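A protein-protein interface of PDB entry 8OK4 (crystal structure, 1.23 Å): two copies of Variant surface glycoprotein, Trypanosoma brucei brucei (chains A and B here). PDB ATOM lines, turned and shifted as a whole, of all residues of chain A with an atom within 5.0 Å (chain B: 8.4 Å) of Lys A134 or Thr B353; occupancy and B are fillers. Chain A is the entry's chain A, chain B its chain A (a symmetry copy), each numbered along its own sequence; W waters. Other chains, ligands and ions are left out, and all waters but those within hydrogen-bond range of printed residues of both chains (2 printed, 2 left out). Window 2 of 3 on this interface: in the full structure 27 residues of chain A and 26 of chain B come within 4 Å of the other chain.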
ATOM      1  N   GLU A 130      21.967  11.752 -22.105  1.00  0.00           N
ATOM      2  CA  GLU A 130      22.535  12.544 -21.021  1.00  0.00           C
ATOM      3  C   GLU A 130      23.895  12.004 -20.605  1.00  0.00           C
ATOM      4  O   GLU A 130      24.826  12.779 -20.361  1.00  0.00           O
ATOM      5  CB  GLU A 130      21.552  12.578 -19.845  1.00  0.00           C
ATOM      6  CG  GLU A 130      20.269  13.354 -20.191  1.00  0.00           C
ATOM      7  CD  GLU A 130      19.105  13.116 -19.246  1.00  0.00           C
ATOM      8  OE1 GLU A 130      19.291  12.467 -18.190  1.00  0.00           O
ATOM      9  OE2 GLU A 130      17.996  13.604 -19.565  1.00  0.00           O
ATOM     10  N   ALA A 131      24.038  10.675 -20.546  1.00  0.00           N
ATOM     11  CA  ALA A 131      25.319  10.070 -20.190  1.00  0.00           C
ATOM     12  C   ALA A 131      26.404  10.442 -21.190  1.00  0.00           C
ATOM     13  O   ALA A 131      27.521  10.811 -20.804  1.00  0.00           O
ATOM     14  CB  ALA A 131      25.174   8.551 -20.116  1.00  0.00           C
ATOM     15  N   VAL A 132      26.095  10.346 -22.486  1.00  0.00           N
ATOM     16  CA  VAL A 132      27.070  10.708 -23.511  1.00  0.00           C
ATOM     17  C   VAL A 132      27.474  12.172 -23.376  1.00  0.00           C
ATOM     18  O   VAL A 132      28.657  12.515 -23.479  1.00  0.00           O
ATOM     19  CB  VAL A 132      26.524  10.378 -24.913  1.00  0.00           C
ATOM     20  CG1 VAL A 132      27.459  10.916 -25.987  1.00  0.00           C
ATOM     21  CG2 VAL A 132      26.336   8.881 -25.078  1.00  0.00           C
ATOM     22  N   ALA A 133      26.505  13.060 -23.161  1.00  0.00           N
ATOM     23  CA  ALA A 133      26.827  14.478 -23.026  1.00  0.00           C
ATOM     24  C   ALA A 133      27.682  14.736 -21.792  1.00  0.00           C
ATOM     25  O   ALA A 133      28.640  15.515 -21.842  1.00  0.00           O
ATOM     26  CB  ALA A 133      25.539  15.296 -22.968  1.00  0.00           C
ATOM     27  N   LYS A 134      27.358  14.087 -20.676  1.00  0.00           N
ATOM     28  CA  LYS A 134      28.105  14.320 -19.446  1.00  0.00           C
ATOM     29  C   LYS A 134      29.524  13.762 -19.517  1.00  0.00           C
ATOM     30  O   LYS A 134      30.434  14.280 -18.856  1.00  0.00           O
ATOM     31  CB  LYS A 134      27.366  13.669 -18.283  1.00  0.00           C
ATOM     32  CG  LYS A 134      26.088  14.375 -17.895  1.00  0.00           C
ATOM     33  CD  LYS A 134      25.365  13.604 -16.807  1.00  0.00           C
ATOM     34  CE  LYS A 134      23.985  14.164 -16.538  1.00  0.00           C
ATOM     35  NZ  LYS A 134      24.035  15.618 -16.239  1.00  0.00           N
ATOM     36  N   ALA A 135      29.749  12.720 -20.297  1.00  0.00           N
ATOM     37  CA  ALA A 135      31.049  12.018 -20.349  1.00  0.00           C
ATOM     38  C   ALA A 135      32.021  12.830 -21.194  1.00  0.00           C
ATOM     39  O   ALA A 135      33.174  12.425 -21.282  1.00  0.00           O
ATOM     40  CB  ALA A 135      30.849  10.639 -20.893  1.00  0.00           C
ATOM     41  N   GLN A 136      31.582  13.936 -21.768  1.00  0.00           N
ATOM     42  CA  GLN A 136      32.491  14.850 -22.499  1.00  0.00           C
ATOM     43  C   GLN A 136      33.024  15.922 -21.548  1.00  0.00           C
ATOM     44  O   GLN A 136      32.236  16.510 -20.814  1.00  0.00           O
ATOM     45  CB  GLN A 136      31.760  15.571 -23.614  1.00  0.00           C
ATOM     46  CG  GLN A 136      30.796  14.705 -24.404  1.00  0.00           C
ATOM     47  CD  GLN A 136      31.523  13.654 -25.202  1.00  0.00           C
ATOM     48  OE1 GLN A 136      32.490  13.946 -25.901  1.00  0.00           O
ATOM     49  NE2 GLN A 136      31.066  12.418 -25.092  1.00  0.00           N
ATOM     50  N   PRO A 347      31.658  13.613 -13.788  1.00  0.00           N
ATOM     51  CA  PRO A 347      31.040  12.660 -14.721  1.00  0.00           C
ATOM     52  C   PRO A 347      31.066  11.233 -14.209  1.00  0.00           C
ATOM     53  O   PRO A 347      30.134  10.468 -14.493  1.00  0.00           O
ATOM     54  CB  PRO A 347      31.857  12.845 -16.008  1.00  0.00           C
ATOM     55  CG  PRO A 347      33.129  13.550 -15.568  1.00  0.00           C
ATOM     56  CD  PRO A 347      32.724  14.406 -14.426  1.00  0.00           C
ATOM     57  N   ASP A 350      28.095  11.059 -12.026  1.00  0.00           N
ATOM     58  CA  ASP A 350      26.909  11.200 -12.861  1.00  0.00           C
ATOM     59  C   ASP A 350      26.564   9.902 -13.583  1.00  0.00           C
ATOM     60  O   ASP A 350      25.390   9.525 -13.674  1.00  0.00           O
ATOM     61  CB  ASP A 350      27.137  12.300 -13.898  1.00  0.00           C
ATOM     62  CG  ASP A 350      26.964  13.703 -13.335  1.00  0.00           C
ATOM     63  OD1 ASP A 350      26.407  13.868 -12.230  1.00  0.00           O
ATOM     64  OD2 ASP A 350      27.385  14.652 -14.021  1.00  0.00           O
ATOM     65  N   LEU A 351      27.574   9.213 -14.114  1.00  0.00           N
ATOM     66  CA  LEU A 351      27.321   8.008 -14.895  1.00  0.00           C
ATOM     67  C   LEU A 351      26.919   6.841 -14.000  1.00  0.00           C
ATOM     68  O   LEU A 351      26.087   6.013 -14.389  1.00  0.00           O
ATOM     69  CB  LEU A 351      28.561   7.681 -15.723  1.00  0.00           C
ATOM     70  CG  LEU A 351      28.636   8.359 -17.096  1.00  0.00           C
ATOM     71  CD1 LEU A 351      28.256   9.833 -17.056  1.00  0.00           C
ATOM     72  CD2 LEU A 351      30.042   8.202 -17.662  1.00  0.00           C
ATOM     73  N   ILE A 354      23.287   7.485 -13.353  1.00  0.00           N
ATOM     74  CA  ILE A 354      22.455   7.144 -14.505  1.00  0.00           C
ATOM     75  C   ILE A 354      22.277   5.637 -14.617  1.00  0.00           C
ATOM     76  O   ILE A 354      21.173   5.147 -14.898  1.00  0.00           O
ATOM     77  CB  ILE A 354      23.024   7.766 -15.793  1.00  0.00           C
ATOM     78  CG1 ILE A 354      22.805   9.276 -15.759  1.00  0.00           C
ATOM     79  CG2 ILE A 354      22.368   7.130 -17.035  1.00  0.00           C
ATOM     80  CD1 ILE A 354      23.546  10.033 -16.821  1.00  0.00           C
ATOM     81  N   GLU B  37      28.060  30.244 -20.324  1.00  0.00           N
ATOM     82  CA  GLU B  37      27.196  29.119 -20.645  1.00  0.00           C
ATOM     83  C   GLU B  37      25.770  29.378 -20.191  1.00  0.00           C
ATOM     84  O   GLU B  37      24.823  29.074 -20.919  1.00  0.00           O
ATOM     85  CB  GLU B  37      27.732  27.837 -20.014  1.00  0.00           C
ATOM     86  CG  GLU B  37      29.038  27.370 -20.623  1.00  0.00           C
ATOM     87  CD  GLU B  37      30.194  28.308 -20.324  1.00  0.00           C
ATOM     88  OE1 GLU B  37      30.322  28.755 -19.168  1.00  0.00           O
ATOM     89  OE2 GLU B  37      30.941  28.635 -21.269  1.00  0.00           O
ATOM     90  N   ILE B  41      22.479  29.508 -22.648  1.00  0.00           N
ATOM     91  CA  ILE B  41      21.278  28.699 -22.442  1.00  0.00           C
ATOM     92  C   ILE B  41      20.034  29.585 -22.374  1.00  0.00           C
ATOM     93  O   ILE B  41      19.003  29.282 -22.986  1.00  0.00           O
ATOM     94  CB  ILE B  41      21.443  27.819 -21.185  1.00  0.00           C
ATOM     95  CG1 ILE B  41      22.567  26.799 -21.372  1.00  0.00           C
ATOM     96  CG2 ILE B  41      20.135  27.119 -20.866  1.00  0.00           C
ATOM     97  CD1 ILE B  41      23.079  26.195 -20.072  1.00  0.00           C
ATOM     98  N   LEU B 127      15.317  22.214 -19.493  1.00  0.00           N
ATOM     99  CA  LEU B 127      16.768  22.314 -19.378  1.00  0.00           C
ATOM    100  C   LEU B 127      17.193  23.683 -18.872  1.00  0.00           C
ATOM    101  O   LEU B 127      18.141  23.799 -18.085  1.00  0.00           O
ATOM    102  CB  LEU B 127      17.428  22.067 -20.733  1.00  0.00           C
ATOM    103  CG  LEU B 127      17.429  20.633 -21.240  1.00  0.00           C
ATOM    104  CD1 LEU B 127      17.954  20.639 -22.670  1.00  0.00           C
ATOM    105  CD2 LEU B 127      18.209  19.671 -20.367  1.00  0.00           C
ATOM    106  N   GLU B 130      16.565  23.980 -15.181  1.00  0.00           N
ATOM    107  CA  GLU B 130      17.590  23.206 -14.491  1.00  0.00           C
ATOM    108  C   GLU B 130      18.914  23.957 -14.463  1.00  0.00           C
ATOM    109  O   GLU B 130      19.603  23.965 -13.438  1.00  0.00           O
ATOM    110  CB  GLU B 130      17.728  21.834 -15.159  1.00  0.00           C
ATOM    111  CG  GLU B 130      16.469  20.971 -14.965  1.00  0.00           C
ATOM    112  CD  GLU B 130      16.363  19.776 -15.896  1.00  0.00           C
ATOM    113  OE1 GLU B 130      17.340  19.473 -16.621  1.00  0.00           O
ATOM    114  OE2 GLU B 130      15.291  19.128 -15.883  1.00  0.00           O
ATOM    115  N   LYS B 134      20.924  25.021 -11.123  1.00  0.00           N
ATOM    116  CA  LYS B 134      22.268  24.511 -10.875  1.00  0.00           C
ATOM    117  C   LYS B 134      23.293  25.632 -10.724  1.00  0.00           C
ATOM    118  O   LYS B 134      24.303  25.467 -10.027  1.00  0.00           O
ATOM    119  CB  LYS B 134      22.677  23.606 -12.030  1.00  0.00           C
ATOM    120  CG  LYS B 134      21.949  22.283 -12.062  1.00  0.00           C
ATOM    121  CD  LYS B 134      22.336  21.493 -13.297  1.00  0.00           C
ATOM    122  CE  LYS B 134      21.477  20.259 -13.473  1.00  0.00           C
ATOM    123  NZ  LYS B 134      21.483  19.411 -12.254  1.00  0.00           N
ATOM    124  N   LYS B 346      31.574  21.999 -10.577  1.00  0.00           N
ATOM    125  CA  LYS B 346      30.380  21.182 -10.787  1.00  0.00           C
ATOM    126  C   LYS B 346      29.335  21.898 -11.633  1.00  0.00           C
ATOM    127  O   LYS B 346      28.950  21.373 -12.695  1.00  0.00           O
ATOM    128  CB  LYS B 346      29.827  20.719  -9.437  1.00  0.00           C
ATOM    129  N   PRO B 347      28.817  23.059 -11.233  1.00  0.00           N
ATOM    130  CA  PRO B 347      27.890  23.778 -12.119  1.00  0.00           C
ATOM    131  C   PRO B 347      28.500  24.110 -13.466  1.00  0.00           C
ATOM    132  O   PRO B 347      27.780  24.122 -14.473  1.00  0.00           O
ATOM    133  CB  PRO B 347      27.523  25.029 -11.306  1.00  0.00           C
ATOM    134  CG  PRO B 347      28.598  25.133 -10.239  1.00  0.00           C
ATOM    135  CD  PRO B 347      28.979  23.733  -9.931  1.00  0.00           C
ATOM    136  N   GLN B 348      29.811  24.360 -13.528  1.00  0.00           N
ATOM    137  CA  GLN B 348      30.440  24.606 -14.821  1.00  0.00           C
ATOM    138  C   GLN B 348      30.229  23.420 -15.757  1.00  0.00           C
ATOM    139  O   GLN B 348      29.794  23.584 -16.904  1.00  0.00           O
ATOM    140  CB  GLN B 348      31.929  24.901 -14.640  1.00  0.00           C
ATOM    141  CG  GLN B 348      32.644  25.171 -15.955  1.00  0.00           C
ATOM    142  CD  GLN B 348      34.133  25.398 -15.790  1.00  0.00           C
ATOM    143  OE1 GLN B 348      34.696  26.320 -16.377  1.00  0.00           O
ATOM    144  NE2 GLN B 348      34.780  24.549 -14.997  1.00  0.00           N
ATOM    145  N   HIS B 349      30.517  22.207 -15.275  1.00  0.00           N
ATOM    146  CA  HIS B 349      30.334  21.017 -16.103  1.00  0.00           C
ATOM    147  C   HIS B 349      28.857  20.796 -16.409  1.00  0.00           C
ATOM    148  O   HIS B 349      28.487  20.428 -17.533  1.00  0.00           O
ATOM    149  CB  HIS B 349      30.933  19.790 -15.402  1.00  0.00           C
ATOM    150  CG  HIS B 349      30.690  18.496 -16.124  1.00  0.00           C
ATOM    151  ND1 HIS B 349      29.715  17.597 -15.743  1.00  0.00           N
ATOM    152  CD2 HIS B 349      31.293  17.954 -17.211  1.00  0.00           C
ATOM    153  CE1 HIS B 349      29.725  16.562 -16.565  1.00  0.00           C
ATOM    154  NE2 HIS B 349      30.677  16.751 -17.460  1.00  0.00           N
ATOM    155  N   ASP B 350      28.001  21.015 -15.413  1.00  0.00           N
ATOM    156  CA  ASP B 350      26.569  20.833 -15.617  1.00  0.00           C
ATOM    157  C   ASP B 350      26.035  21.726 -16.733  1.00  0.00           C
ATOM    158  O   ASP B 350      25.220  21.289 -17.552  1.00  0.00           O
ATOM    159  CB  ASP B 350      25.819  21.152 -14.324  1.00  0.00           C
ATOM    160  CG  ASP B 350      25.866  20.020 -13.306  1.00  0.00           C
ATOM    161  OD1 ASP B 350      26.228  18.880 -13.659  1.00  0.00           O
ATOM    162  OD2 ASP B 350      25.521  20.284 -12.140  1.00  0.00           O
ATOM    163  N   LEU B 351      26.476  22.983 -16.770  1.00  0.00           N
ATOM    164  CA  LEU B 351      25.949  23.925 -17.750  1.00  0.00           C
ATOM    165  C   LEU B 351      26.490  23.633 -19.145  1.00  0.00           C
ATOM    166  O   LEU B 351      25.774  23.804 -20.140  1.00  0.00           O
ATOM    167  CB  LEU B 351      26.281  25.347 -17.304  1.00  0.00           C
ATOM    168  CG  LEU B 351      25.260  26.002 -16.368  1.00  0.00           C
ATOM    169  CD1 LEU B 351      24.783  25.070 -15.260  1.00  0.00           C
ATOM    170  CD2 LEU B 351      25.862  27.261 -15.761  1.00  0.00           C
ATOM    171  N   LYS B 352      27.746  23.191 -19.242  1.00  0.00           N
ATOM    172  CA  LYS B 352      28.264  22.745 -20.534  1.00  0.00           C
ATOM    173  C   LYS B 352      27.478  21.545 -21.050  1.00  0.00           C
ATOM    174  O   LYS B 352      27.184  21.459 -22.251  1.00  0.00           O
ATOM    175  CB  LYS B 352      29.748  22.404 -20.431  1.00  0.00           C
ATOM    176  CG  LYS B 352      30.613  23.625 -20.280  1.00  0.00           C
ATOM    177  CD  LYS B 352      32.088  23.269 -20.206  1.00  0.00           C
ATOM    178  CE  LYS B 352      32.913  24.508 -19.941  1.00  0.00           C
ATOM    179  NZ  LYS B 352      32.652  25.543 -20.981  1.00  0.00           N
ATOM    180  N   THR B 353      27.153  20.599 -20.155  1.00  0.00           N
ATOM    181  CA  THR B 353      26.333  19.444 -20.520  1.00  0.00           C
ATOM    182  C   THR B 353      24.961  19.880 -21.026  1.00  0.00           C
ATOM    183  O   THR B 353      24.467  19.363 -22.034  1.00  0.00           O
ATOM    184  CB  THR B 353      26.141  18.526 -19.308  1.00  0.00           C
ATOM    185  OG1 THR B 353      27.406  18.007 -18.883  1.00  0.00           O
ATOM    186  CG2 THR B 353      25.199  17.360 -19.640  1.00  0.00           C
ATOM    187  N   ILE B 354      24.320  20.815 -20.318  1.00  0.00           N
ATOM    188  CA  ILE B 354      22.989  21.274 -20.715  1.00  0.00           C
ATOM    189  C   ILE B 354      23.034  21.947 -22.079  1.00  0.00           C
ATOM    190  O   ILE B 354      22.152  21.732 -22.922  1.00  0.00           O
ATOM    191  CB  ILE B 354      22.379  22.180 -19.631  1.00  0.00           C
ATOM    192  CG1 ILE B 354      22.005  21.329 -18.420  1.00  0.00           C
ATOM    193  CG2 ILE B 354      21.156  22.938 -20.186  1.00  0.00           C
ATOM    194  CD1 ILE B 354      21.649  22.119 -17.195  1.00  0.00           C
ATOM    195  N   LEU B 355      24.063  22.761 -22.324  1.00  0.00           N
ATOM    196  CA  LEU B 355      24.198  23.392 -23.632  1.00  0.00           C
ATOM    197  C   LEU B 355      24.339  22.344 -24.728  1.00  0.00           C
ATOM    198  O   LEU B 355      23.756  22.486 -25.806  1.00  0.00           O
ATOM    199  CB  LEU B 355      25.390  24.342 -23.613  1.00  0.00           C
ATOM    200  CG  LEU B 355      25.460  25.442 -24.662  1.00  0.00           C
ATOM    201  CD1 LEU B 355      24.162  26.233 -24.728  1.00  0.00           C
ATOM    202  CD2 LEU B 355      26.646  26.347 -24.359  1.00  0.00           C
ATOM    203  N   THR B 356      25.105  21.285 -24.469  1.00  0.00           N
ATOM    204  CA  THR B 356      25.240  20.204 -25.441  1.00  0.00           C
ATOM    205  C   THR B 356      23.888  19.574 -25.753  1.00  0.00           C
ATOM    206  O   THR B 356      23.548  19.340 -26.920  1.00  0.00           O
ATOM    207  CB  THR B 356      26.221  19.158 -24.893  1.00  0.00           C
ATOM    208  OG1 THR B 356      27.530  19.728 -24.818  1.00  0.00           O
ATOM    209  CG2 THR B 356      26.267  17.918 -25.776  1.00  0.00           C
ATOM    210  N   LEU B 357      23.115  19.261 -24.712  1.00  0.00           N
ATOM    211  CA  LEU B 357      21.814  18.623 -24.905  1.00  0.00           C
ATOM    212  C   LEU B 357      20.836  19.558 -25.612  1.00  0.00           C
ATOM    213  O   LEU B 357      20.039  19.121 -26.457  1.00  0.00           O
ATOM    214  CB  LEU B 357      21.255  18.181 -23.548  1.00  0.00           C
ATOM    215  CG  LEU B 357      21.998  17.040 -22.852  1.00  0.00           C
ATOM    216  CD1 LEU B 357      21.502  16.878 -21.424  1.00  0.00           C
ATOM    217  CD2 LEU B 357      21.844  15.757 -23.641  1.00  0.00           C
ATOM    218  N   ALA B 358      20.890  20.849 -25.283  1.00  0.00           N
ATOM    219  CA  ALA B 358      19.945  21.809 -25.839  1.00  0.00           C
ATOM    220  C   ALA B 358      20.197  22.054 -27.317  1.00  0.00           C
ATOM    221  O   ALA B 358      19.277  22.479 -28.031  1.00  0.00           O
ATOM    222  CB  ALA B 358      20.048  23.124 -25.068  1.00  0.00           C
ATOM    223  N   LYS B 359      21.422  21.798 -27.780  1.00  0.00           N
ATOM    224  CA  LYS B 359      21.794  21.917 -29.182  1.00  0.00           C
ATOM    225  C   LYS B 359      21.724  20.584 -29.920  1.00  0.00           C
ATOM    226  O   LYS B 359      22.182  20.503 -31.063  1.00  0.00           O
ATOM    227  CB  LYS B 359      23.199  22.531 -29.296  1.00  0.00           C
ATOM    228  CG  LYS B 359      23.249  24.011 -28.901  1.00  0.00           C
ATOM    229  CD  LYS B 359      24.613  24.667 -29.177  1.00  0.00           C
ATOM    230  CE  LYS B 359      25.721  23.997 -28.395  1.00  0.00           C
ATOM    231  NZ  LYS B 359      26.966  24.825 -28.331  1.00  0.00           N
ATOM    232  N   ASP B 360      21.151  19.536 -29.296  1.00  0.00           N
ATOM    233  CA  ASP B 360      21.088  18.193 -29.865  1.00  0.00           C
ATOM    234  C   ASP B 360      19.667  17.964 -30.374  1.00  0.00           C
ATOM    235  O   ASP B 360      18.761  17.670 -29.574  1.00  0.00           O
ATOM    236  CB  ASP B 360      21.460  17.158 -28.796  1.00  0.00           C
ATOM    237  CG  ASP B 360      21.375  15.714 -29.286  1.00  0.00           C
ATOM    238  OD1 ASP B 360      20.861  15.451 -30.390  1.00  0.00           O
ATOM    239  OD2 ASP B 360      21.866  14.824 -28.555  1.00  0.00           O
ATOM    240  N   TYR B 363      17.846  14.693 -29.109  1.00  0.00           N
ATOM    241  CA  TYR B 363      17.480  14.694 -27.695  1.00  0.00           C
ATOM    242  C   TYR B 363      16.233  15.535 -27.458  1.00  0.00           C
ATOM    243  O   TYR B 363      15.352  15.157 -26.680  1.00  0.00           O
ATOM    244  CB  TYR B 363      18.634  15.245 -26.850  1.00  0.00           C
ATOM    245  CG  TYR B 363      18.326  15.305 -25.374  1.00  0.00           C
ATOM    246  CD1 TYR B 363      18.382  14.163 -24.592  1.00  0.00           C
ATOM    247  CD2 TYR B 363      17.984  16.499 -24.758  1.00  0.00           C
ATOM    248  CE1 TYR B 363      18.104  14.207 -23.247  1.00  0.00           C
ATOM    249  CE2 TYR B 363      17.700  16.553 -23.407  1.00  0.00           C
ATOM    250  CZ  TYR B 363      17.764  15.405 -22.654  1.00  0.00           C
ATOM    251  OH  TYR B 363      17.483  15.459 -21.309  1.00  0.00           O
HETATM  252  O   HOH W   1      25.942  17.296 -15.759  1.00  0.00           O
HETATM  253  O   HOH W   2      23.681  18.912 -16.169  1.00  0.00           O
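Hydrophobic or aromatic side chains of chain B within 4 Å of the printed part of chain A: His B349, Leu B357 and Tyr B363.
Of the 11 printed residues of chain A, 5 touch a printed residue of chain B.
Printed residues of chain A that touch a printed residue of chain B: Glu A130, Ala A133, Lys A134, Gln A136 and Asp A350.
Hydrophobic or aromatic side chains of chain A within 4 Å of the printed part of chain B: Ala A133.
Among the printed residues, 9 pairs touch across the chains.
O of Val A132 sits at hydrogen-bond distance from NE2 of Gln A136 (2.9 Å).
O of His B349 sits at hydrogen-bond distance from OG1 of Thr B353, 3.0 Å away.
The side-chain hydroxyl (OG1) of Thr B356 is in hydrogen-bond range of the backbone carbonyl oxygen (O) of Lys B352 (3.1 Å).
The side-chain carboxylate of Asp B360 lies within hydrogen-bond range of the backbone NH of Tyr B363, at 3.4 Å.
Positions printed for both chains: 130, 134, 347, 350, 351 and 354.
OH of Tyr B363 lies within hydrogen-bond range of OE2 of Glu A130.
O of Lys A134 sits at hydrogen-bond distance from NE2 of His B349, 2.8 Å away.
Among the printed residues, pairs that only touch across the chains: Lys A134 with Thr B353 (3.6 Å), Gln A136 with His B349 (3.7 Å), Ala A133 with Leu B357 (3.8 Å), Ala A133 with Thr B356 (3.9 Å), Ala A133 with Thr B353 (3.9 Å), Glu A130 with Leu B357 (3.9 Å) and Asp A350 with His B349 (3.9 Å).
Water W1 lies within hydrogen-bond range of the side-chain amino group (NZ) of Lys A134 (2.6 Å), the side-chain carboxylate (OD1) of Asp B350 (2.6 Å) and the side-chain carboxylate (OD2) of Asp A350 (3.5 Å).
Water W2 lies within hydrogen-bond range of the backbone carbonyl oxygen (O) of Asp B350 and the side-chain amino group (NZ) of Lys A134.
Printed residues of chain B within 4 Å of Glu A130: Leu B357 (3.9 Å) and Tyr B363 (2.6 Å).
Of the printed residues of chain B, Lys A134 touches His B349 (2.8 Å) and Thr B353 (3.6 Å).
No residue of chain B comes within 4 Å of Ala A135.
Printed residues of chain B within 4 Å of Gln A136: His B349 (3.7 Å).
Leu A351 touches none of the printed residues of chain B.
Thr B353 touches two residues of chain A.
The nearest printed residue of chain A that does not touch Thr B356 is Gln A136 (5.7 Å).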
